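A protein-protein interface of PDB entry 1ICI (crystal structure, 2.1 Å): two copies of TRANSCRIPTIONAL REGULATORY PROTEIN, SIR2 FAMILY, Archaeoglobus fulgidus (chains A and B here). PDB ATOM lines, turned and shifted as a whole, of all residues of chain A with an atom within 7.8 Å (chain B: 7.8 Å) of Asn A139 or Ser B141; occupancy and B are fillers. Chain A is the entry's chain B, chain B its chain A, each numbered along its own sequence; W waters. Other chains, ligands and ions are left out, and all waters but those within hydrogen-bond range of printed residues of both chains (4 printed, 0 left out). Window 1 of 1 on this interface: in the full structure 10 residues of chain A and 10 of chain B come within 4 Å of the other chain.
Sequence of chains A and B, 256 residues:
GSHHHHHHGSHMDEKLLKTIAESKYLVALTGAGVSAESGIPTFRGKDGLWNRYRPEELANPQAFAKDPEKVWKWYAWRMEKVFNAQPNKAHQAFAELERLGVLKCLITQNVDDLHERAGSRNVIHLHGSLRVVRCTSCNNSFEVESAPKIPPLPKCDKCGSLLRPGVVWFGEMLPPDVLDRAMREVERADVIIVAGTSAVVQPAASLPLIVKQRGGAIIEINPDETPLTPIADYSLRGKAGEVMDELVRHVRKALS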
ATOM      1  N   VAL A 133      -0.218  18.847  27.559  1.00  0.00           N
ATOM      2  CA  VAL A 133       1.038  18.485  26.916  1.00  0.00           C
ATOM      3  C   VAL A 133       1.673  19.830  26.644  1.00  0.00           C
ATOM      4  O   VAL A 133       0.970  20.797  26.378  1.00  0.00           O
ATOM      5  CB  VAL A 133       0.784  17.712  25.590  1.00  0.00           C
ATOM      6  CG1 VAL A 133       2.053  17.635  24.766  1.00  0.00           C
ATOM      7  CG2 VAL A 133       0.278  16.307  25.908  1.00  0.00           C
ATOM      8  N   ARG A 134       2.988  19.917  26.763  1.00  0.00           N
ATOM      9  CA  ARG A 134       3.655  21.179  26.505  1.00  0.00           C
ATOM     10  C   ARG A 134       5.035  21.001  25.900  1.00  0.00           C
ATOM     11  O   ARG A 134       5.705  19.995  26.136  1.00  0.00           O
ATOM     12  CB  ARG A 134       3.763  22.000  27.784  1.00  0.00           C
ATOM     13  CG  ARG A 134       4.730  21.495  28.811  1.00  0.00           C
ATOM     14  CD  ARG A 134       5.147  22.668  29.699  1.00  0.00           C
ATOM     15  NE  ARG A 134       6.084  22.260  30.735  1.00  0.00           N
ATOM     16  CZ  ARG A 134       5.727  21.590  31.825  1.00  0.00           C
ATOM     17  NH1 ARG A 134       4.450  21.264  32.002  1.00  0.00           N
ATOM     18  NH2 ARG A 134       6.637  21.248  32.736  1.00  0.00           N
ATOM     19  N   CYS A 135       5.458  21.989  25.119  1.00  0.00           N
ATOM     20  CA  CYS A 135       6.762  21.941  24.485  1.00  0.00           C
ATOM     21  C   CYS A 135       7.894  22.169  25.469  1.00  0.00           C
ATOM     22  O   CYS A 135       7.899  23.152  26.203  1.00  0.00           O
ATOM     23  CB  CYS A 135       6.865  22.979  23.362  1.00  0.00           C
ATOM     24  SG  CYS A 135       8.524  22.989  22.632  1.00  0.00           S
ATOM     25  N   THR A 136       8.865  21.265  25.469  1.00  0.00           N
ATOM     26  CA  THR A 136      10.007  21.380  26.368  1.00  0.00           C
ATOM     27  C   THR A 136      10.954  22.510  25.973  1.00  0.00           C
ATOM     28  O   THR A 136      11.855  22.853  26.730  1.00  0.00           O
ATOM     29  CB  THR A 136      10.832  20.084  26.396  1.00  0.00           C
ATOM     30  OG1 THR A 136      11.207  19.735  25.057  1.00  0.00           O
ATOM     31  CG2 THR A 136      10.033  18.949  27.030  1.00  0.00           C
ATOM     32  N   SER A 137      10.753  23.083  24.791  1.00  0.00           N
ATOM     33  CA  SER A 137      11.626  24.152  24.318  1.00  0.00           C
ATOM     34  C   SER A 137      11.002  25.537  24.266  1.00  0.00           C
ATOM     35  O   SER A 137      11.550  26.484  24.834  1.00  0.00           O
ATOM     36  CB  SER A 137      12.162  23.815  22.931  1.00  0.00           C
ATOM     37  OG  SER A 137      12.668  24.980  22.302  1.00  0.00           O
ATOM     38  N   CYS A 138       9.871  25.654  23.572  1.00  0.00           N
ATOM     39  CA  CYS A 138       9.177  26.933  23.429  1.00  0.00           C
ATOM     40  C   CYS A 138       8.096  27.131  24.491  1.00  0.00           C
ATOM     41  O   CYS A 138       7.450  28.176  24.540  1.00  0.00           O
ATOM     42  CB  CYS A 138       8.534  27.035  22.050  1.00  0.00           C
ATOM     43  SG  CYS A 138       6.968  26.180  21.923  1.00  0.00           S
ATOM     44  N   ASN A 139       7.885  26.113  25.316  1.00  0.00           N
ATOM     45  CA  ASN A 139       6.899  26.170  26.392  1.00  0.00           C
ATOM     46  C   ASN A 139       5.424  26.269  26.000  1.00  0.00           C
ATOM     47  O   ASN A 139       4.575  26.425  26.875  1.00  0.00           O
ATOM     48  CB  ASN A 139       7.239  27.319  27.342  1.00  0.00           C
ATOM     49  CG  ASN A 139       8.665  27.247  27.842  1.00  0.00           C
ATOM     50  OD1 ASN A 139       9.097  26.221  28.382  1.00  0.00           O
ATOM     51  ND2 ASN A 139       9.410  28.336  27.666  1.00  0.00           N
ATOM     52  N   ASN A 140       5.092  26.205  24.715  1.00  0.00           N
ATOM     53  CA  ASN A 140       3.672  26.265  24.396  1.00  0.00           C
ATOM     54  C   ASN A 140       2.992  25.102  25.130  1.00  0.00           C
ATOM     55  O   ASN A 140       3.555  24.008  25.253  1.00  0.00           O
ATOM     56  CB  ASN A 140       3.402  26.142  22.906  1.00  0.00           C
ATOM     57  CG  ASN A 140       1.927  26.250  22.592  1.00  0.00           C
ATOM     58  OD1 ASN A 140       1.277  27.212  23.000  1.00  0.00           O
ATOM     59  ND2 ASN A 140       1.383  25.263  21.883  1.00  0.00           N
ATOM     60  N   SER A 141       1.783  25.343  25.616  1.00  0.00           N
ATOM     61  CA  SER A 141       1.052  24.333  26.363  1.00  0.00           C
ATOM     62  C   SER A 141      -0.394  24.266  25.870  1.00  0.00           C
ATOM     63  O   SER A 141      -1.022  25.303  25.623  1.00  0.00           O
ATOM     64  CB  SER A 141       1.101  24.684  27.853  1.00  0.00           C
ATOM     65  OG  SER A 141       0.443  23.708  28.632  1.00  0.00           O
ATOM     66  N   PHE A 142      -0.919  23.049  25.738  1.00  0.00           N
ATOM     67  CA  PHE A 142      -2.283  22.860  25.256  1.00  0.00           C
ATOM     68  C   PHE A 142      -2.846  21.547  25.772  1.00  0.00           C
ATOM     69  O   PHE A 142      -2.108  20.726  26.317  1.00  0.00           O
ATOM     70  CB  PHE A 142      -2.290  22.863  23.721  1.00  0.00           C
ATOM     71  CG  PHE A 142      -1.382  21.830  23.112  1.00  0.00           C
ATOM     72  CD1 PHE A 142      -1.874  20.582  22.734  1.00  0.00           C
ATOM     73  CD2 PHE A 142      -0.028  22.098  22.936  1.00  0.00           C
ATOM     74  CE1 PHE A 142      -1.022  19.609  22.188  1.00  0.00           C
ATOM     75  CE2 PHE A 142       0.834  21.135  22.392  1.00  0.00           C
ATOM     76  CZ  PHE A 142       0.337  19.890  22.019  1.00  0.00           C
ATOM     77  N   CYS A 156       6.389  19.572  18.982  1.00  0.00           N
ATOM     78  CA  CYS A 156       5.727  20.876  18.946  1.00  0.00           C
ATOM     79  C   CYS A 156       5.473  21.424  17.537  1.00  0.00           C
ATOM     80  O   CYS A 156       6.385  21.494  16.718  1.00  0.00           O
ATOM     81  CB  CYS A 156       6.562  21.877  19.749  1.00  0.00           C
ATOM     82  SG  CYS A 156       5.879  23.539  19.856  1.00  0.00           S
ATOM     83  N   LYS A 158       4.613  24.519  16.736  1.00  0.00           N
ATOM     84  CA  LYS A 158       5.193  25.844  16.660  1.00  0.00           C
ATOM     85  C   LYS A 158       6.718  25.919  16.559  1.00  0.00           C
ATOM     86  O   LYS A 158       7.247  26.922  16.077  1.00  0.00           O
ATOM     87  CB  LYS A 158       4.696  26.659  17.849  1.00  0.00           C
ATOM     88  CG  LYS A 158       3.215  26.424  18.120  1.00  0.00           C
ATOM     89  CD  LYS A 158       2.536  27.645  18.688  1.00  0.00           C
ATOM     90  CE  LYS A 158       2.394  28.730  17.629  1.00  0.00           C
ATOM     91  NZ  LYS A 158       1.751  29.945  18.192  1.00  0.00           N
ATOM     92  N   CYS A 159       7.428  24.880  16.995  1.00  0.00           N
ATOM     93  CA  CYS A 159       8.886  24.910  16.918  1.00  0.00           C
ATOM     94  C   CYS A 159       9.522  23.548  16.633  1.00  0.00           C
ATOM     95  O   CYS A 159      10.748  23.426  16.589  1.00  0.00           O
ATOM     96  CB  CYS A 159       9.478  25.511  18.202  1.00  0.00           C
ATOM     97  SG  CYS A 159       9.731  24.368  19.585  1.00  0.00           S
ATOM     98  N   SER A 161      10.062  21.090  18.411  1.00  0.00           N
ATOM     99  CA  SER A 161      10.773  20.445  19.507  1.00  0.00           C
ATOM    100  C   SER A 161       9.959  19.334  20.162  1.00  0.00           C
ATOM    101  O   SER A 161       8.778  19.136  19.852  1.00  0.00           O
ATOM    102  CB  SER A 161      11.185  21.478  20.559  1.00  0.00           C
ATOM    103  OG  SER A 161      12.045  22.441  19.989  1.00  0.00           O
ATOM    104  N   LEU A 162      10.610  18.621  21.073  1.00  0.00           N
ATOM    105  CA  LEU A 162      10.007  17.504  21.788  1.00  0.00           C
ATOM    106  C   LEU A 162       8.982  17.951  22.827  1.00  0.00           C
ATOM    107  O   LEU A 162       9.254  18.814  23.653  1.00  0.00           O
ATOM    108  CB  LEU A 162      11.112  16.695  22.478  1.00  0.00           C
ATOM    109  CG  LEU A 162      10.730  15.598  23.477  1.00  0.00           C
ATOM    110  CD1 LEU A 162      10.045  14.443  22.760  1.00  0.00           C
ATOM    111  CD2 LEU A 162      11.987  15.113  24.197  1.00  0.00           C
ATOM    112  N   LEU A 163       7.796  17.364  22.771  1.00  0.00           N
ATOM    113  CA  LEU A 163       6.759  17.688  23.736  1.00  0.00           C
ATOM    114  C   LEU A 163       6.938  16.764  24.952  1.00  0.00           C
ATOM    115  O   LEU A 163       7.700  15.789  24.904  1.00  0.00           O
ATOM    116  CB  LEU A 163       5.382  17.485  23.102  1.00  0.00           C
ATOM    117  CG  LEU A 163       5.050  18.418  21.928  1.00  0.00           C
ATOM    118  CD1 LEU A 163       4.024  17.766  21.013  1.00  0.00           C
ATOM    119  CD2 LEU A 163       4.541  19.753  22.460  1.00  0.00           C
ATOM    120  N   ARG B 131      -2.133  35.451  18.949  1.00  0.00           N
ATOM    121  CA  ARG B 131      -2.758  34.189  19.350  1.00  0.00           C
ATOM    122  C   ARG B 131      -2.158  33.659  20.640  1.00  0.00           C
ATOM    123  O   ARG B 131      -2.768  32.867  21.351  1.00  0.00           O
ATOM    124  CB  ARG B 131      -2.553  33.107  18.283  1.00  0.00           C
ATOM    125  CG  ARG B 131      -3.545  33.129  17.162  1.00  0.00           C
ATOM    126  CD  ARG B 131      -4.962  32.850  17.659  1.00  0.00           C
ATOM    127  NE  ARG B 131      -5.913  33.020  16.565  1.00  0.00           N
ATOM    128  CZ  ARG B 131      -7.234  32.952  16.681  1.00  0.00           C
ATOM    129  NH1 ARG B 131      -7.796  32.709  17.860  1.00  0.00           N
ATOM    130  NH2 ARG B 131      -7.989  33.162  15.611  1.00  0.00           N
ATOM    131  N   VAL B 132      -0.946  34.085  20.929  1.00  0.00           N
ATOM    132  CA  VAL B 132      -0.256  33.598  22.103  1.00  0.00           C
ATOM    133  C   VAL B 132      -0.424  34.532  23.272  1.00  0.00           C
ATOM    134  O   VAL B 132      -0.382  35.758  23.120  1.00  0.00           O
ATOM    135  CB  VAL B 132       1.259  33.447  21.817  1.00  0.00           C
ATOM    136  CG1 VAL B 132       2.006  33.116  23.099  1.00  0.00           C
ATOM    137  CG2 VAL B 132       1.488  32.367  20.739  1.00  0.00           C
ATOM    138  N   VAL B 133      -0.656  33.940  24.432  1.00  0.00           N
ATOM    139  CA  VAL B 133      -0.744  34.685  25.657  1.00  0.00           C
ATOM    140  C   VAL B 133       0.310  33.972  26.512  1.00  0.00           C
ATOM    141  O   VAL B 133       0.320  32.737  26.577  1.00  0.00           O
ATOM    142  CB  VAL B 133      -2.143  34.576  26.293  1.00  0.00           C
ATOM    143  CG1 VAL B 133      -2.097  35.109  27.719  1.00  0.00           C
ATOM    144  CG2 VAL B 133      -3.160  35.397  25.464  1.00  0.00           C
ATOM    145  N   ARG B 134       1.226  34.733  27.113  1.00  0.00           N
ATOM    146  CA  ARG B 134       2.278  34.150  27.938  1.00  0.00           C
ATOM    147  C   ARG B 134       2.480  34.907  29.239  1.00  0.00           C
ATOM    148  O   ARG B 134       2.092  36.061  29.364  1.00  0.00           O
ATOM    149  CB  ARG B 134       3.599  34.074  27.166  1.00  0.00           C
ATOM    150  CG  ARG B 134       4.293  35.403  26.910  1.00  0.00           C
ATOM    151  CD  ARG B 134       5.583  35.131  26.169  1.00  0.00           C
ATOM    152  NE  ARG B 134       6.399  36.325  25.977  1.00  0.00           N
ATOM    153  CZ  ARG B 134       7.027  36.970  26.955  1.00  0.00           C
ATOM    154  NH1 ARG B 134       6.934  36.538  28.209  1.00  0.00           N
ATOM    155  NH2 ARG B 134       7.758  38.041  26.672  1.00  0.00           N
ATOM    156  N   CYS B 135       3.092  34.244  30.214  1.00  0.00           N
ATOM    157  CA  CYS B 135       3.307  34.870  31.512  1.00  0.00           C
ATOM    158  C   CYS B 135       4.483  35.836  31.514  1.00  0.00           C
ATOM    159  O   CYS B 135       5.482  35.608  30.837  1.00  0.00           O
ATOM    160  CB  CYS B 135       3.537  33.805  32.598  1.00  0.00           C
ATOM    161  SG  CYS B 135       3.749  34.516  34.249  1.00  0.00           S
ATOM    162  N   CYS B 138       6.824  33.478  34.732  1.00  0.00           N
ATOM    163  CA  CYS B 138       7.323  32.121  34.501  1.00  0.00           C
ATOM    164  C   CYS B 138       7.256  31.853  32.987  1.00  0.00           C
ATOM    165  O   CYS B 138       6.928  32.765  32.221  1.00  0.00           O
ATOM    166  CB  CYS B 138       6.502  31.090  35.293  1.00  0.00           C
ATOM    167  SG  CYS B 138       4.810  30.748  34.710  1.00  0.00           S
ATOM    168  N   ASN B 139       7.574  30.631  32.553  1.00  0.00           N
ATOM    169  CA  ASN B 139       7.562  30.294  31.120  1.00  0.00           C
ATOM    170  C   ASN B 139       6.227  29.826  30.543  1.00  0.00           C
ATOM    171  O   ASN B 139       6.146  29.444  29.378  1.00  0.00           O
ATOM    172  CB  ASN B 139       8.605  29.215  30.815  1.00  0.00           C
ATOM    173  CG  ASN B 139      10.007  29.676  31.099  1.00  0.00           C
ATOM    174  OD1 ASN B 139      10.419  30.746  30.652  1.00  0.00           O
ATOM    175  ND2 ASN B 139      10.756  28.876  31.843  1.00  0.00           N
ATOM    176  N   ASN B 140       5.186  29.838  31.360  1.00  0.00           N
ATOM    177  CA  ASN B 140       3.875  29.411  30.912  1.00  0.00           C
ATOM    178  C   ASN B 140       3.484  30.158  29.623  1.00  0.00           C
ATOM    179  O   ASN B 140       3.600  31.381  29.544  1.00  0.00           O
ATOM    180  CB  ASN B 140       2.876  29.668  32.041  1.00  0.00           C
ATOM    181  CG  ASN B 140       1.489  29.171  31.718  1.00  0.00           C
ATOM    182  OD1 ASN B 140       1.325  28.141  31.065  1.00  0.00           O
ATOM    183  ND2 ASN B 140       0.478  29.897  32.186  1.00  0.00           N
ATOM    184  N   SER B 141       3.048  29.411  28.610  1.00  0.00           N
ATOM    185  CA  SER B 141       2.633  29.997  27.331  1.00  0.00           C
ATOM    186  C   SER B 141       1.529  29.136  26.696  1.00  0.00           C
ATOM    187  O   SER B 141       1.558  27.905  26.781  1.00  0.00           O
ATOM    188  CB  SER B 141       3.830  30.085  26.382  1.00  0.00           C
ATOM    189  OG  SER B 141       3.537  30.916  25.281  1.00  0.00           O
ATOM    190  N   PHE B 142       0.553  29.786  26.072  1.00  0.00           N
ATOM    191  CA  PHE B 142      -0.557  29.066  25.457  1.00  0.00           C
ATOM    192  C   PHE B 142      -1.282  29.925  24.433  1.00  0.00           C
ATOM    193  O   PHE B 142      -1.126  31.146  24.416  1.00  0.00           O
ATOM    194  CB  PHE B 142      -1.533  28.605  26.543  1.00  0.00           C
ATOM    195  CG  PHE B 142      -2.122  29.730  27.368  1.00  0.00           C
ATOM    196  CD1 PHE B 142      -3.320  30.344  26.988  1.00  0.00           C
ATOM    197  CD2 PHE B 142      -1.501  30.143  28.553  1.00  0.00           C
ATOM    198  CE1 PHE B 142      -3.902  31.348  27.772  1.00  0.00           C
ATOM    199  CE2 PHE B 142      -2.071  31.153  29.357  1.00  0.00           C
ATOM    200  CZ  PHE B 142      -3.275  31.757  28.966  1.00  0.00           C
ATOM    201  N   GLU B 143      -2.082  29.289  23.584  1.00  0.00           N
ATOM    202  CA  GLU B 143      -2.824  30.023  22.563  1.00  0.00           C
ATOM    203  C   GLU B 143      -4.292  30.200  22.934  1.00  0.00           C
ATOM    204  O   GLU B 143      -4.882  29.350  23.588  1.00  0.00           O
ATOM    205  CB  GLU B 143      -2.679  29.319  21.212  1.00  0.00           C
ATOM    206  CG  GLU B 143      -1.252  29.341  20.706  1.00  0.00           C
ATOM    207  CD  GLU B 143      -1.107  28.735  19.333  1.00  0.00           C
ATOM    208  OE1 GLU B 143      -1.427  27.537  19.181  1.00  0.00           O
ATOM    209  OE2 GLU B 143      -0.673  29.452  18.408  1.00  0.00           O
ATOM    210  N   CYS B 156      -1.588  34.336  35.375  1.00  0.00           N
ATOM    211  CA  CYS B 156      -1.051  32.999  35.134  1.00  0.00           C
ATOM    212  C   CYS B 156      -1.536  31.973  36.171  1.00  0.00           C
ATOM    213  O   CYS B 156      -1.441  32.214  37.377  1.00  0.00           O
ATOM    214  CB  CYS B 156       0.473  33.082  35.161  1.00  0.00           C
ATOM    215  SG  CYS B 156       1.318  31.527  34.949  1.00  0.00           S
ATOM    216  N   LYS B 158      -0.150  29.258  36.848  1.00  0.00           N
ATOM    217  CA  LYS B 158       1.011  28.501  37.332  1.00  0.00           C
ATOM    218  C   LYS B 158       1.755  29.280  38.427  1.00  0.00           C
ATOM    219  O   LYS B 158       2.135  28.702  39.455  1.00  0.00           O
ATOM    220  CB  LYS B 158       1.998  28.198  36.197  1.00  0.00           C
ATOM    221  CG  LYS B 158       1.394  27.432  35.024  1.00  0.00           C
ATOM    222  CD  LYS B 158       0.837  26.076  35.441  1.00  0.00           C
ATOM    223  CE  LYS B 158       0.128  25.424  34.266  1.00  0.00           C
ATOM    224  NZ  LYS B 158      -0.626  24.217  34.675  1.00  0.00           N
ATOM    225  N   LEU B 163      -0.276  37.949  32.974  1.00  0.00           N
ATOM    226  CA  LEU B 163      -0.039  37.381  31.655  1.00  0.00           C
ATOM    227  C   LEU B 163       0.086  38.585  30.717  1.00  0.00           C
ATOM    228  O   LEU B 163      -0.326  39.694  31.061  1.00  0.00           O
ATOM    229  CB  LEU B 163      -1.212  36.503  31.224  1.00  0.00           C
ATOM    230  CG  LEU B 163      -1.383  35.163  31.939  1.00  0.00           C
ATOM    231  CD1 LEU B 163      -2.763  34.580  31.600  1.00  0.00           C
ATOM    232  CD2 LEU B 163      -0.296  34.209  31.491  1.00  0.00           C
ATOM    233  N   ARG B 164       0.658  38.364  29.539  1.00  0.00           N
ATOM    234  CA  ARG B 164       0.849  39.422  28.548  1.00  0.00           C
ATOM    235  C   ARG B 164       0.706  38.838  27.145  1.00  0.00           C
ATOM    236  O   ARG B 164       0.769  37.612  26.962  1.00  0.00           O
ATOM    237  CB  ARG B 164       2.258  40.002  28.678  1.00  0.00           C
ATOM    238  CG  ARG B 164       3.337  38.948  28.452  1.00  0.00           C
ATOM    239  CD  ARG B 164       4.716  39.549  28.270  1.00  0.00           C
ATOM    240  NE  ARG B 164       4.940  40.000  26.894  1.00  0.00           N
ATOM    241  CZ  ARG B 164       5.987  40.729  26.516  1.00  0.00           C
ATOM    242  NH1 ARG B 164       6.906  41.096  27.406  1.00  0.00           N
ATOM    243  NH2 ARG B 164       6.126  41.080  25.247  1.00  0.00           N
ATOM    244  N   GLY B 166       1.651  37.518  23.560  1.00  0.00           N
ATOM    245  CA  GLY B 166       2.875  36.829  23.168  1.00  0.00           C
ATOM    246  C   GLY B 166       3.575  37.446  21.973  1.00  0.00           C
ATOM    247  O   GLY B 166       3.938  36.751  21.020  1.00  0.00           O
HETATM  248  O   HOH W   1       2.690  29.462  23.117  1.00  0.00           O
HETATM  249  O   HOH W   2      -1.466  25.628  20.948  1.00  0.00           O
HETATM  250  O   HOH W   3       3.940  26.291  29.303  1.00  0.00           O
HETATM  251  O   HOH W   4      -2.194  26.283  23.537  1.00  0.00           O
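The backbone NH of Ser A141 is in hydrogen-bond range of the backbone carbonyl oxygen of Ser B141, at 2.8 Å.
The side-chain amino group of Lys A158 is in salt-bridge range of the side-chain carboxylate of Glu B143 (2.5 Å).
The backbone carbonyl oxygen of Asn A139 lies close to the backbone carbonyl oxygen of Ser B141, at 3.4 Å.
O of Val B132 sits at hydrogen-bond distance from N of Gly B166 (2.7 Å).
The backbone carbonyl oxygen (O) of Phe B142 sits at hydrogen-bond distance from the backbone NH (N) of Val B133.
The backbone carbonyl oxygen of Asn A140 lies within hydrogen-bond range of the backbone NH of Cys A135, at 2.8 Å.
N of Asn A140 sits close to SG of Cys A138 (3.4 Å).
The side-chain sulfur (SG) of Cys A156 sits close to the backbone NH (N) of Lys A158 (3.5 Å).
Asn A139 touches Asn B139.
Ser B141 touches Asn A140.
CA of Phe B142 touches OD1 of Asn A140 (3.6 Å).
OD1 of Asn A140 touches N of Glu B143 (3.99 Å).
Ser A141 touches Phe B142 (O to CB, 3.5 Å).
Lys A158 touches Val B132 (NZ to CG2, 3.5 Å).
Of chain A, only Asn A139, Asn A140 and Ser A141 come within 4 Å of Ser B141.
No residue of chain B comes within 4 Å of Cys A138.
Of the printed residues of chain A, Glu B143 touches Asn A140 (3.99 Å) and Lys A158 (2.5 Å).
Of the printed residues of chain B, Asn A140 touches Ser B141, Phe B142 and Glu B143.
Arg B164 touches none of the printed residues of chain A.
Of the 16 printed residues of chain B, 5 touch a printed residue of chain A.
Printed residues of chain A that touch a printed residue of chain B: Asn A139, Asn A140, Ser A141 and Lys A158.
Among the printed residues, Asp or Glu carboxylates within 4 Å of a Lys or Arg side-chain nitrogen of the other chain: Lys A158 with Glu B143 (2.5 Å).
Asn A140 touches Ser B141, but with the chains exchanged Ser A141 does not touch Asn B140 (4.7 Å).
Asn A140 touches Phe B142, but with the chains exchanged Phe A142 does not touch Asn B140 (7.7 Å).
Ser B141 touches its own counterpart, Ser A141.
Ser A141 touches Phe B142, but with the chains exchanged Phe A142 does not touch Ser B141 (5.6 Å).
Of the 9 pairs that touch across the chains among the printed residues, 2 have their exchanged pair printed and touching as well.
Water W3 bridges O of Asn A139 (2.5 Å) and N of Ser B141 (3.3 Å).
Water W4 lies within hydrogen-bond range of O of Ser A141 and N of Glu B143.
Water W2 lies within hydrogen-bond range of OE1 of Glu B143 (2.6 Å) and ND2 of Asn A140 (3.0 Å).
Water W1 lies within hydrogen-bond range of OD1 of Asn A140 and OG of Ser B141.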
